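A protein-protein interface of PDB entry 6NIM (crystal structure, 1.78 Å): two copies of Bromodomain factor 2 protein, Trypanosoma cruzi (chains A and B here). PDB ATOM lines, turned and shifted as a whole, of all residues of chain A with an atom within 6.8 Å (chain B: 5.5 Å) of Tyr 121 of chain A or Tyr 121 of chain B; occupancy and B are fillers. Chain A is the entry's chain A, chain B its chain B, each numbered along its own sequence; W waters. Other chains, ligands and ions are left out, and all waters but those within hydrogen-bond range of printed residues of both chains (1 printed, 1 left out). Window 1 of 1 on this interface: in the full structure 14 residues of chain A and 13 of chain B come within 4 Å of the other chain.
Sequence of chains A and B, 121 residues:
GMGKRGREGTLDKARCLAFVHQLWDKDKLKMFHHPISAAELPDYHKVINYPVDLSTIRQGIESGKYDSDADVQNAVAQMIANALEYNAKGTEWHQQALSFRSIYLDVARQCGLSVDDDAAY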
ATOM      1  N   GLN A  73     -17.596  25.558  11.002  1.00  0.00           N
ATOM      2  CA  GLN A  73     -16.118  25.668  11.102  1.00  0.00           C
ATOM      3  C   GLN A  73     -15.598  26.703  10.102  1.00  0.00           C
ATOM      4  O   GLN A  73     -14.737  27.486  10.479  1.00  0.00           O
ATOM      5  CB  GLN A  73     -15.453  24.315  10.895  1.00  0.00           C
ATOM      6  CG  GLN A  73     -15.770  23.380  12.033  1.00  0.00           C
ATOM      7  CD  GLN A  73     -15.233  22.004  11.797  1.00  0.00           C
ATOM      8  OE1 GLN A  73     -14.123  21.840  11.285  1.00  0.00           O
ATOM      9  NE2 GLN A  73     -16.004  21.026  12.245  1.00  0.00           N
ATOM     10  N   ASN A  74     -16.146  26.726   8.891  1.00  0.00           N
ATOM     11  CA  ASN A  74     -15.746  27.673   7.818  1.00  0.00           C
ATOM     12  C   ASN A  74     -16.128  29.102   8.232  1.00  0.00           C
ATOM     13  O   ASN A  74     -15.372  30.017   7.914  1.00  0.00           O
ATOM     14  CB  ASN A  74     -16.317  27.194   6.478  1.00  0.00           C
ATOM     15  CG  ASN A  74     -15.615  25.930   6.008  1.00  0.00           C
ATOM     16  OD1 ASN A  74     -14.528  25.575   6.491  1.00  0.00           O
ATOM     17  ND2 ASN A  74     -16.214  25.226   5.068  1.00  0.00           N
ATOM     18  N   VAL A  76     -16.307  30.215  11.378  1.00  0.00           N
ATOM     19  CA  VAL A  76     -15.288  30.568  12.398  1.00  0.00           C
ATOM     20  C   VAL A  76     -13.966  30.894  11.688  1.00  0.00           C
ATOM     21  O   VAL A  76     -13.301  31.907  12.031  1.00  0.00           O
ATOM     22  CB  VAL A  76     -15.126  29.409  13.395  1.00  0.00           C
ATOM     23  CG1 VAL A  76     -13.882  29.576  14.245  1.00  0.00           C
ATOM     24  CG2 VAL A  76     -16.362  29.266  14.258  1.00  0.00           C
ATOM     25  N   ALA A  77     -13.579  30.092  10.700  1.00  0.00           N
ATOM     26  CA  ALA A  77     -12.333  30.360   9.933  1.00  0.00           C
ATOM     27  C   ALA A  77     -12.420  31.757   9.298  1.00  0.00           C
ATOM     28  O   ALA A  77     -11.439  32.565   9.353  1.00  0.00           O
ATOM     29  CB  ALA A  77     -12.138  29.265   8.919  1.00  0.00           C
ATOM     30  N   GLN A  78     -13.578  32.126   8.735  1.00  0.00           N
ATOM     31  CA  GLN A  78     -13.703  33.429   8.032  1.00  0.00           C
ATOM     32  C   GLN A  78     -13.565  34.556   9.050  1.00  0.00           C
ATOM     33  O   GLN A  78     -12.912  35.571   8.760  1.00  0.00           O
ATOM     34  CB  GLN A  78     -15.030  33.553   7.269  1.00  0.00           C
ATOM     35  CG  GLN A  78     -15.162  34.907   6.587  1.00  0.00           C
ATOM     36  CD  GLN A  78     -14.212  34.974   5.432  1.00  0.00           C
ATOM     37  OE1 GLN A  78     -14.331  34.157   4.523  1.00  0.00           O
ATOM     38  NE2 GLN A  78     -13.269  35.918   5.469  1.00  0.00           N
ATOM     39  N   ILE A  80     -11.819  34.473  11.807  1.00  0.00           N
ATOM     40  CA  ILE A  80     -10.373  34.558  12.181  1.00  0.00           C
ATOM     41  C   ILE A  80      -9.620  35.235  11.030  1.00  0.00           C
ATOM     42  O   ILE A  80      -8.787  36.103  11.306  1.00  0.00           O
ATOM     43  CB  ILE A  80      -9.837  33.152  12.516  1.00  0.00           C
ATOM     44  CG1 ILE A  80     -10.539  32.589  13.768  1.00  0.00           C
ATOM     45  CG2 ILE A  80      -8.327  33.174  12.668  1.00  0.00           C
ATOM     46  CD1 ILE A  80     -10.293  31.149  14.038  1.00  0.00           C
ATOM     47  N   ALA A  81      -9.854  34.818   9.775  1.00  0.00           N
ATOM     48  CA  ALA A  81      -9.171  35.408   8.593  1.00  0.00           C
ATOM     49  C   ALA A  81      -9.423  36.918   8.562  1.00  0.00           C
ATOM     50  O   ALA A  81      -8.489  37.688   8.290  1.00  0.00           O
ATOM     51  CB  ALA A  81      -9.647  34.712   7.313  1.00  0.00           C
ATOM     52  N   ASN A  82     -10.647  37.349   8.873  1.00  0.00           N
ATOM     53  CA  ASN A  82     -11.017  38.785   8.860  1.00  0.00           C
ATOM     54  C   ASN A  82     -10.057  39.544   9.784  1.00  0.00           C
ATOM     55  O   ASN A  82      -9.576  40.640   9.417  1.00  0.00           O
ATOM     56  CB  ASN A  82     -12.488  38.977   9.231  1.00  0.00           C
ATOM     57  CG  ASN A  82     -13.461  38.488   8.171  1.00  0.00           C
ATOM     58  OD1 ASN A  82     -13.089  38.225   7.027  1.00  0.00           O
ATOM     59  ND2 ASN A  82     -14.733  38.388   8.539  1.00  0.00           N
ATOM     60  N   LEU A  84      -7.090  38.580  10.969  1.00  0.00           N
ATOM     61  CA  LEU A  84      -5.685  38.503  10.469  1.00  0.00           C
ATOM     62  C   LEU A  84      -5.484  39.515   9.331  1.00  0.00           C
ATOM     63  O   LEU A  84      -4.409  40.169   9.312  1.00  0.00           O
ATOM     64  CB  LEU A  84      -5.362  37.071  10.047  1.00  0.00           C
ATOM     65  CG  LEU A  84      -5.141  36.143  11.233  1.00  0.00           C
ATOM     66  CD1 LEU A  84      -5.132  34.703  10.797  1.00  0.00           C
ATOM     67  CD2 LEU A  84      -3.870  36.533  12.011  1.00  0.00           C
ATOM     68  N   GLU A  85      -6.485  39.713   8.469  1.00  0.00           N
ATOM     69  CA  GLU A  85      -6.385  40.716   7.370  1.00  0.00           C
ATOM     70  C   GLU A  85      -6.455  42.140   7.932  1.00  0.00           C
ATOM     71  O   GLU A  85      -5.689  43.013   7.478  1.00  0.00           O
ATOM     72  CB  GLU A  85      -7.512  40.576   6.338  1.00  0.00           C
ATOM     73  CG  GLU A  85      -7.533  39.278   5.573  1.00  0.00           C
ATOM     74  CD  GLU A  85      -8.848  39.029   4.824  1.00  0.00           C
ATOM     75  OE1 GLU A  85      -9.370  39.996   4.211  1.00  0.00           O
ATOM     76  OE2 GLU A  85      -9.374  37.880   4.866  1.00  0.00           O
ATOM     77  N   ALA A  97      -5.579  36.457  16.935  1.00  0.00           N
ATOM     78  CA  ALA A  97      -6.154  35.833  15.727  1.00  0.00           C
ATOM     79  C   ALA A  97      -5.199  34.757  15.205  1.00  0.00           C
ATOM     80  O   ALA A  97      -5.701  33.722  14.759  1.00  0.00           O
ATOM     81  CB  ALA A  97      -6.454  36.892  14.728  1.00  0.00           C
ATOM     82  N   ARG A 101      -6.354  30.944  14.813  1.00  0.00           N
ATOM     83  CA  ARG A 101      -6.164  30.136  13.577  1.00  0.00           C
ATOM     84  C   ARG A 101      -5.512  28.797  13.946  1.00  0.00           C
ATOM     85  O   ARG A 101      -5.878  27.766  13.393  1.00  0.00           O
ATOM     86  CB  ARG A 101      -5.319  30.850  12.530  1.00  0.00           C
ATOM     87  CG  ARG A 101      -5.223  30.041  11.248  1.00  0.00           C
ATOM     88  CD  ARG A 101      -4.542  30.817  10.146  1.00  0.00           C
ATOM     89  NE  ARG A 101      -4.637  30.009   8.943  1.00  0.00           N
ATOM     90  CZ  ARG A 101      -4.283  30.401   7.728  1.00  0.00           C
ATOM     91  NH1 ARG A 101      -3.780  31.611   7.536  1.00  0.00           N
ATOM     92  NH2 ARG A 101      -4.405  29.552   6.715  1.00  0.00           N
ATOM     93  N   TYR A 104      -8.361  26.607  16.514  1.00  0.00           N
ATOM     94  CA  TYR A 104      -9.846  26.546  16.387  1.00  0.00           C
ATOM     95  C   TYR A 104     -10.230  25.104  16.049  1.00  0.00           C
ATOM     96  O   TYR A 104     -11.245  24.600  16.598  1.00  0.00           O
ATOM     97  CB  TYR A 104     -10.448  27.623  15.467  1.00  0.00           C
ATOM     98  CG  TYR A 104     -10.364  27.351  13.982  1.00  0.00           C
ATOM     99  CD1 TYR A 104      -9.165  27.493  13.307  1.00  0.00           C
ATOM    100  CD2 TYR A 104     -11.459  26.919  13.264  1.00  0.00           C
ATOM    101  CE1 TYR A 104      -9.058  27.210  11.957  1.00  0.00           C
ATOM    102  CE2 TYR A 104     -11.383  26.645  11.909  1.00  0.00           C
ATOM    103  CZ  TYR A 104     -10.174  26.801  11.242  1.00  0.00           C
ATOM    104  OH  TYR A 104     -10.052  26.517   9.905  1.00  0.00           O
ATOM    105  N   LEU A 105      -9.452  24.407  15.195  1.00  0.00           N
ATOM    106  CA  LEU A 105      -9.810  23.020  14.844  1.00  0.00           C
ATOM    107  C   LEU A 105      -9.558  22.108  16.050  1.00  0.00           C
ATOM    108  O   LEU A 105     -10.319  21.161  16.256  1.00  0.00           O
ATOM    109  CB  LEU A 105      -8.987  22.532  13.649  1.00  0.00           C
ATOM    110  CG  LEU A 105      -9.227  23.264  12.338  1.00  0.00           C
ATOM    111  CD1 LEU A 105      -8.337  22.644  11.267  1.00  0.00           C
ATOM    112  CD2 LEU A 105     -10.689  23.245  11.912  1.00  0.00           C
ATOM    113  N   ASP A 116     -11.853  18.567   8.755  1.00  0.00           N
ATOM    114  CA  ASP A 116     -11.158  18.215   7.484  1.00  0.00           C
ATOM    115  C   ASP A 116      -9.839  18.992   7.480  1.00  0.00           C
ATOM    116  O   ASP A 116      -9.816  20.141   7.035  1.00  0.00           O
ATOM    117  CB  ASP A 116     -12.107  18.507   6.320  1.00  0.00           C
ATOM    118  CG  ASP A 116     -11.571  18.071   4.976  1.00  0.00           C
ATOM    119  OD1 ASP A 116     -10.327  17.896   4.853  1.00  0.00           O
ATOM    120  OD2 ASP A 116     -12.401  17.892   4.094  1.00  0.00           O
ATOM    121  N   ASP A 117      -8.784  18.412   8.033  1.00  0.00           N
ATOM    122  CA  ASP A 117      -7.494  19.121   8.217  1.00  0.00           C
ATOM    123  C   ASP A 117      -6.957  19.628   6.871  1.00  0.00           C
ATOM    124  O   ASP A 117      -6.477  20.772   6.827  1.00  0.00           O
ATOM    125  CB  ASP A 117      -6.463  18.234   8.911  1.00  0.00           C
ATOM    126  CG  ASP A 117      -6.683  18.234  10.407  1.00  0.00           C
ATOM    127  OD1 ASP A 117      -6.821  19.335  10.968  1.00  0.00           O
ATOM    128  OD2 ASP A 117      -6.812  17.147  10.957  1.00  0.00           O
ATOM    129  N   ASP A 118      -7.019  18.827   5.818  1.00  0.00           N
ATOM    130  CA  ASP A 118      -6.472  19.254   4.495  1.00  0.00           C
ATOM    131  C   ASP A 118      -7.227  20.483   3.982  1.00  0.00           C
ATOM    132  O   ASP A 118      -6.566  21.368   3.378  1.00  0.00           O
ATOM    133  CB  ASP A 118      -6.516  18.136   3.450  1.00  0.00           C
ATOM    134  CG  ASP A 118      -5.449  17.074   3.612  1.00  0.00           C
ATOM    135  OD1 ASP A 118      -4.558  17.248   4.478  1.00  0.00           O
ATOM    136  OD2 ASP A 118      -5.519  16.091   2.876  1.00  0.00           O
ATOM    137  N   ALA A 119      -8.555  20.531   4.136  1.00  0.00           N
ATOM    138  CA  ALA A 119      -9.388  21.610   3.556  1.00  0.00           C
ATOM    139  C   ALA A 119      -9.370  22.870   4.433  1.00  0.00           C
ATOM    140  O   ALA A 119      -9.587  23.969   3.908  1.00  0.00           O
ATOM    141  CB  ALA A 119     -10.788  21.137   3.370  1.00  0.00           C
ATOM    142  N   ALA A 120      -9.272  22.687   5.740  1.00  0.00           N
ATOM    143  CA  ALA A 120      -9.551  23.748   6.729  1.00  0.00           C
ATOM    144  C   ALA A 120      -8.563  24.910   6.578  1.00  0.00           C
ATOM    145  O   ALA A 120      -7.339  24.720   6.365  1.00  0.00           O
ATOM    146  CB  ALA A 120      -9.538  23.170   8.128  1.00  0.00           C
ATOM    147  N   TYR A 121      -9.069  26.110   6.774  1.00  0.00           N
ATOM    148  CA  TYR A 121      -8.242  27.328   6.927  1.00  0.00           C
ATOM    149  C   TYR A 121      -7.203  27.097   8.019  1.00  0.00           C
ATOM    150  O   TYR A 121      -7.525  26.575   9.090  1.00  0.00           O
ATOM    151  CB  TYR A 121      -9.142  28.509   7.249  1.00  0.00           C
ATOM    152  CG  TYR A 121      -8.420  29.804   7.442  1.00  0.00           C
ATOM    153  CD1 TYR A 121      -7.891  30.488   6.368  1.00  0.00           C
ATOM    154  CD2 TYR A 121      -8.325  30.375   8.703  1.00  0.00           C
ATOM    155  CE1 TYR A 121      -7.253  31.704   6.543  1.00  0.00           C
ATOM    156  CE2 TYR A 121      -7.728  31.607   8.887  1.00  0.00           C
ATOM    157  CZ  TYR A 121      -7.182  32.272   7.807  1.00  0.00           C
ATOM    158  OH  TYR A 121      -6.553  33.480   7.964  1.00  0.00           O
ATOM    159  OXT TYR A 121      -6.038  27.443   7.783  1.00  0.00           O
ATOM    160  N   ALA B  77      -8.425  30.840  -3.594  1.00  0.00           N
ATOM    161  CA  ALA B  77      -8.424  30.071  -2.335  1.00  0.00           C
ATOM    162  C   ALA B  77      -9.731  29.290  -2.244  1.00  0.00           C
ATOM    163  O   ALA B  77      -9.705  28.102  -1.857  1.00  0.00           O
ATOM    164  CB  ALA B  77      -8.245  30.974  -1.147  1.00  0.00           C
ATOM    165  N   ILE B  80      -9.833  26.275  -4.463  1.00  0.00           N
ATOM    166  CA  ILE B  80      -8.955  25.182  -3.956  1.00  0.00           C
ATOM    167  C   ILE B  80      -9.627  24.496  -2.763  1.00  0.00           C
ATOM    168  O   ILE B  80      -9.644  23.258  -2.744  1.00  0.00           O
ATOM    169  CB  ILE B  80      -7.548  25.727  -3.640  1.00  0.00           C
ATOM    170  CG1 ILE B  80      -6.864  26.288  -4.897  1.00  0.00           C
ATOM    171  CG2 ILE B  80      -6.703  24.689  -2.915  1.00  0.00           C
ATOM    172  CD1 ILE B  80      -5.689  27.189  -4.582  1.00  0.00           C
ATOM    173  N   ALA B  81     -10.163  25.261  -1.804  1.00  0.00           N
ATOM    174  CA  ALA B  81     -10.853  24.748  -0.604  1.00  0.00           C
ATOM    175  C   ALA B  81     -11.999  23.849  -1.056  1.00  0.00           C
ATOM    176  O   ALA B  81     -12.188  22.738  -0.494  1.00  0.00           O
ATOM    177  CB  ALA B  81     -11.347  25.903   0.243  1.00  0.00           C
ATOM    178  N   LEU B  84     -10.682  20.436  -2.041  1.00  0.00           N
ATOM    179  CA  LEU B  84     -10.206  19.678  -0.863  1.00  0.00           C
ATOM    180  C   LEU B  84     -11.410  19.172  -0.051  1.00  0.00           C
ATOM    181  O   LEU B  84     -11.331  18.046   0.436  1.00  0.00           O
ATOM    182  CB  LEU B  84      -9.267  20.560  -0.046  1.00  0.00           C
ATOM    183  CG  LEU B  84      -7.938  20.859  -0.732  1.00  0.00           C
ATOM    184  CD1 LEU B  84      -7.167  21.945   0.038  1.00  0.00           C
ATOM    185  CD2 LEU B  84      -7.109  19.576  -0.880  1.00  0.00           C
ATOM    186  N   ARG B 101      -2.977  24.299  -3.181  1.00  0.00           N
ATOM    187  CA  ARG B 101      -2.989  25.048  -1.900  1.00  0.00           C
ATOM    188  C   ARG B 101      -1.548  25.413  -1.525  1.00  0.00           C
ATOM    189  O   ARG B 101      -1.319  26.534  -1.018  1.00  0.00           O
ATOM    190  CB  ARG B 101      -3.670  24.287  -0.770  1.00  0.00           C
ATOM    191  CG  ARG B 101      -3.802  25.185   0.458  1.00  0.00           C
ATOM    192  CD  ARG B 101      -4.597  24.542   1.552  1.00  0.00           C
ATOM    193  NE  ARG B 101      -4.656  25.475   2.674  1.00  0.00           N
ATOM    194  CZ  ARG B 101      -5.317  25.253   3.802  1.00  0.00           C
ATOM    195  NH1 ARG B 101      -5.980  24.121   3.986  1.00  0.00           N
ATOM    196  NH2 ARG B 101      -5.282  26.163   4.761  1.00  0.00           N
ATOM    197  N   TYR B 104      -0.227  28.206  -4.556  1.00  0.00           N
ATOM    198  CA  TYR B 104      -0.983  29.320  -5.194  1.00  0.00           C
ATOM    199  C   TYR B 104      -0.471  30.676  -4.706  1.00  0.00           C
ATOM    200  O   TYR B 104      -0.501  31.615  -5.519  1.00  0.00           O
ATOM    201  CB  TYR B 104      -2.498  29.174  -5.074  1.00  0.00           C
ATOM    202  CG  TYR B 104      -3.111  29.663  -3.799  1.00  0.00           C
ATOM    203  CD1 TYR B 104      -2.997  28.924  -2.638  1.00  0.00           C
ATOM    204  CD2 TYR B 104      -3.783  30.874  -3.757  1.00  0.00           C
ATOM    205  CE1 TYR B 104      -3.522  29.371  -1.444  1.00  0.00           C
ATOM    206  CE2 TYR B 104      -4.340  31.330  -2.579  1.00  0.00           C
ATOM    207  CZ  TYR B 104      -4.196  30.588  -1.422  1.00  0.00           C
ATOM    208  OH  TYR B 104      -4.676  31.073  -0.240  1.00  0.00           O
ATOM    209  N   LEU B 105      -0.048  30.819  -3.445  1.00  0.00           N
ATOM    210  CA  LEU B 105       0.381  32.156  -2.933  1.00  0.00           C
ATOM    211  C   LEU B 105       1.744  32.506  -3.533  1.00  0.00           C
ATOM    212  O   LEU B 105       1.979  33.702  -3.802  1.00  0.00           O
ATOM    213  CB  LEU B 105       0.479  32.151  -1.407  1.00  0.00           C
ATOM    214  CG  LEU B 105      -0.843  31.934  -0.683  1.00  0.00           C
ATOM    215  CD1 LEU B 105      -0.604  31.791   0.809  1.00  0.00           C
ATOM    216  CD2 LEU B 105      -1.843  33.044  -0.972  1.00  0.00           C
ATOM    217  N   ASP B 118       0.207  35.854   6.886  1.00  0.00           N
ATOM    218  CA  ASP B 118      -0.482  35.381   8.119  1.00  0.00           C
ATOM    219  C   ASP B 118      -1.960  35.069   7.849  1.00  0.00           C
ATOM    220  O   ASP B 118      -2.479  34.112   8.430  1.00  0.00           O
ATOM    221  CB  ASP B 118      -0.374  36.427   9.220  1.00  0.00           C
ATOM    222  CG  ASP B 118       0.961  36.449   9.942  1.00  0.00           C
ATOM    223  OD1 ASP B 118       1.830  35.608   9.596  1.00  0.00           O
ATOM    224  OD2 ASP B 118       1.102  37.269  10.890  1.00  0.00           O
ATOM    225  N   ALA B 119      -2.611  35.839   6.989  1.00  0.00           N
ATOM    226  CA  ALA B 119      -4.078  35.811   6.772  1.00  0.00           C
ATOM    227  C   ALA B 119      -4.458  34.794   5.688  1.00  0.00           C
ATOM    228  O   ALA B 119      -5.621  34.317   5.697  1.00  0.00           O
ATOM    229  CB  ALA B 119      -4.562  37.186   6.401  1.00  0.00           C
ATOM    230  N   ALA B 120      -3.547  34.484   4.765  1.00  0.00           N
ATOM    231  CA  ALA B 120      -3.909  33.763   3.514  1.00  0.00           C
ATOM    232  C   ALA B 120      -4.279  32.318   3.851  1.00  0.00           C
ATOM    233  O   ALA B 120      -3.662  31.693   4.733  1.00  0.00           O
ATOM    234  CB  ALA B 120      -2.792  33.823   2.505  1.00  0.00           C
ATOM    235  N   TYR B 121      -5.281  31.804   3.142  1.00  0.00           N
ATOM    236  CA  TYR B 121      -5.700  30.393   3.189  1.00  0.00           C
ATOM    237  C   TYR B 121      -4.498  29.513   2.854  1.00  0.00           C
ATOM    238  O   TYR B 121      -3.811  29.787   1.828  1.00  0.00           O
ATOM    239  CB  TYR B 121      -6.846  30.176   2.202  1.00  0.00           C
ATOM    240  CG  TYR B 121      -7.230  28.729   2.067  1.00  0.00           C
ATOM    241  CD1 TYR B 121      -7.933  28.104   3.070  1.00  0.00           C
ATOM    242  CD2 TYR B 121      -6.936  28.001   0.925  1.00  0.00           C
ATOM    243  CE1 TYR B 121      -8.348  26.792   2.957  1.00  0.00           C
ATOM    244  CE2 TYR B 121      -7.355  26.687   0.795  1.00  0.00           C
ATOM    245  CZ  TYR B 121      -8.032  26.069   1.823  1.00  0.00           C
ATOM    246  OH  TYR B 121      -8.418  24.769   1.695  1.00  0.00           O
ATOM    247  OXT TYR B 121      -4.180  28.565   3.634  1.00  0.00           O
HETATM  248  O   HOH W   1     -12.455  15.930   1.950  1.00  0.00           O
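O of Asp 118 of chain B is in hydrogen-bond range of NH1 of Arg 101 of chain A, 3.0 Å away.
NH1 of Arg 101 of chain A sits at hydrogen-bond distance from O of Ala 120 of chain B (2.8 Å).
The guanidinium group of Arg 101 of chain A lies within salt-bridge range of the chain-end carboxylate of Tyr 121 of chain B, 3.2 Å away.
The guanidinium group of Arg 101 of chain B sits at hydrogen-bond distance from the backbone carbonyl oxygen of Asp 118 of chain A, at 2.9 Å.
The side-chain hydroxyl (OH) of Tyr 121 of chain B sits at hydrogen-bond distance from the backbone carbonyl oxygen (O) of Ala 119 of chain A (2.6 Å).
The backbone carbonyl oxygen (O) of Ala 120 of chain A sits at hydrogen-bond distance from the guanidinium group (NH1) of Arg 101 of chain B (2.8 Å).
The chain-end carboxylate (OXT) of Tyr 121 of chain A is in salt-bridge range of the guanidinium group (NH2) of Arg 101 of chain B, 3.4 Å away.
The side-chain hydroxyl (OH) of Tyr 121 of chain A is in hydrogen-bond range of the backbone carbonyl oxygen (O) of Ala 119 of chain B, 2.6 Å away.
The guanidinium group (NH2) of Arg 101 of chain A is in salt-bridge range of the chain-end carboxylate (OXT) of Tyr 121 of chain A, 2.9 Å away.
OH of Tyr 104 of chain A lies within hydrogen-bond range of O of Tyr 121 of chain A, at 2.7 Å.
The backbone NH (N) of Ala 119 of chain A is in hydrogen-bond range of the side-chain carboxylate (OD1) of Asp 116 of chain A, 3.3 Å away.
NH2 of Arg 101 of chain B is in salt-bridge range of OXT of Tyr 121 of chain B.
The side-chain hydroxyl (OH) of Tyr 104 of chain B is in hydrogen-bond range of the chain-end carboxylate (O) of Tyr 121 of chain B, 2.6 Å away.
Printed residues of chain A within 4 Å of Tyr 121 of chain B: Arg 101 (3.2 Å), Ala 119 (2.6 Å) and Tyr 121 (3.9 Å).
Of the printed residues of chain B, Glu 85 of chain A touches Ala 119 (3.7 Å).
Of the printed residues of chain A, Ala 119 of chain B touches Leu 84 (3.7 Å), Glu 85 (3.7 Å), Arg 101 (3.7 Å) and Tyr 121 (2.6 Å).
Printed residues of chain A within 4 Å of Arg 101 of chain B: Asp 118, Ala 119, Ala 120 and Tyr 121.
Of the printed residues of chain B, Asp 118 of chain A touches Leu 84 and Arg 101.
Tyr 104 of chain B touches none of the printed residues of chain A.
The nearest residue of chain B that does not touch Tyr 121 of chain A is Ala 120 of chain B (4.02 Å).
The nearest printed residue of chain B that does not touch Arg 101 of chain A is Arg 101 of chain B (4.01 Å).
Arg 101 of chain A touches Asp 118 of chain B, and with the chains exchanged Asp 118 of chain A touches Arg 101 of chain B.
Arg 101 of chain A touches Ala 119 of chain B, and with the chains exchanged Ala 119 of chain A touches Arg 101 of chain B.
Arg 101 of chain A touches Tyr 121 of chain B, and with the chains exchanged Tyr 121 of chain A touches Arg 101 of chain B.
Ala 119 of chain A touches Tyr 121 of chain B, and with the chains exchanged Tyr 121 of chain A touches Ala 119 of chain B.
Water W1 lies within hydrogen-bond range of the backbone carbonyl oxygen (O) of Leu 84 of chain B (2.8 Å) and the side-chain carboxylate (OD2) of Asp 116 of chain A (2.9 Å).
Hydrophobic or aromatic side chains of chain B that line the printed part of chain A: Leu 84, Ala 119 and Tyr 121.
Of the 20 printed residues of chain A, 8 touch a printed residue of chain B.
Printed residues of chain A that touch a printed residue of chain B: Leu 84, Glu 85, Arg 101, Asp 116, Asp 118, Ala 119, Ala 120 and Tyr 121.
Hydrophobic or aromatic side chains of chain A that line the printed part of chain B: Leu 84, Ala 119 and Tyr 121.
Among the printed residues, 17 pairs touch across the chains.
Among the printed residues, no Asp or Glu carboxylate lies within 4 Å of a Lys or Arg side-chain nitrogen of the other chain.
Among the printed residues, pairs that only touch across the chains: Leu 84 of chain A with Asp 118 of chain B (3.6 Å), Leu 84 of chain A with Ala 119 of chain B (3.7 Å), Glu 85 of chain A with Ala 119 of chain B (3.7 Å), Arg 101 of chain A with Ala 119 of chain B (3.7 Å), Asp 116 of chain A with Leu 84 of chain B (3.8 Å), Asp 118 of chain A with Leu 84 of chain B (3.4 Å), Ala 119 of chain A with Leu 84 of chain B (3.8 Å), Ala 119 of chain A with Arg 101 of chain B (3.6 Å) and Tyr 121 of chain A with Tyr 121 of chain B (3.9 Å).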
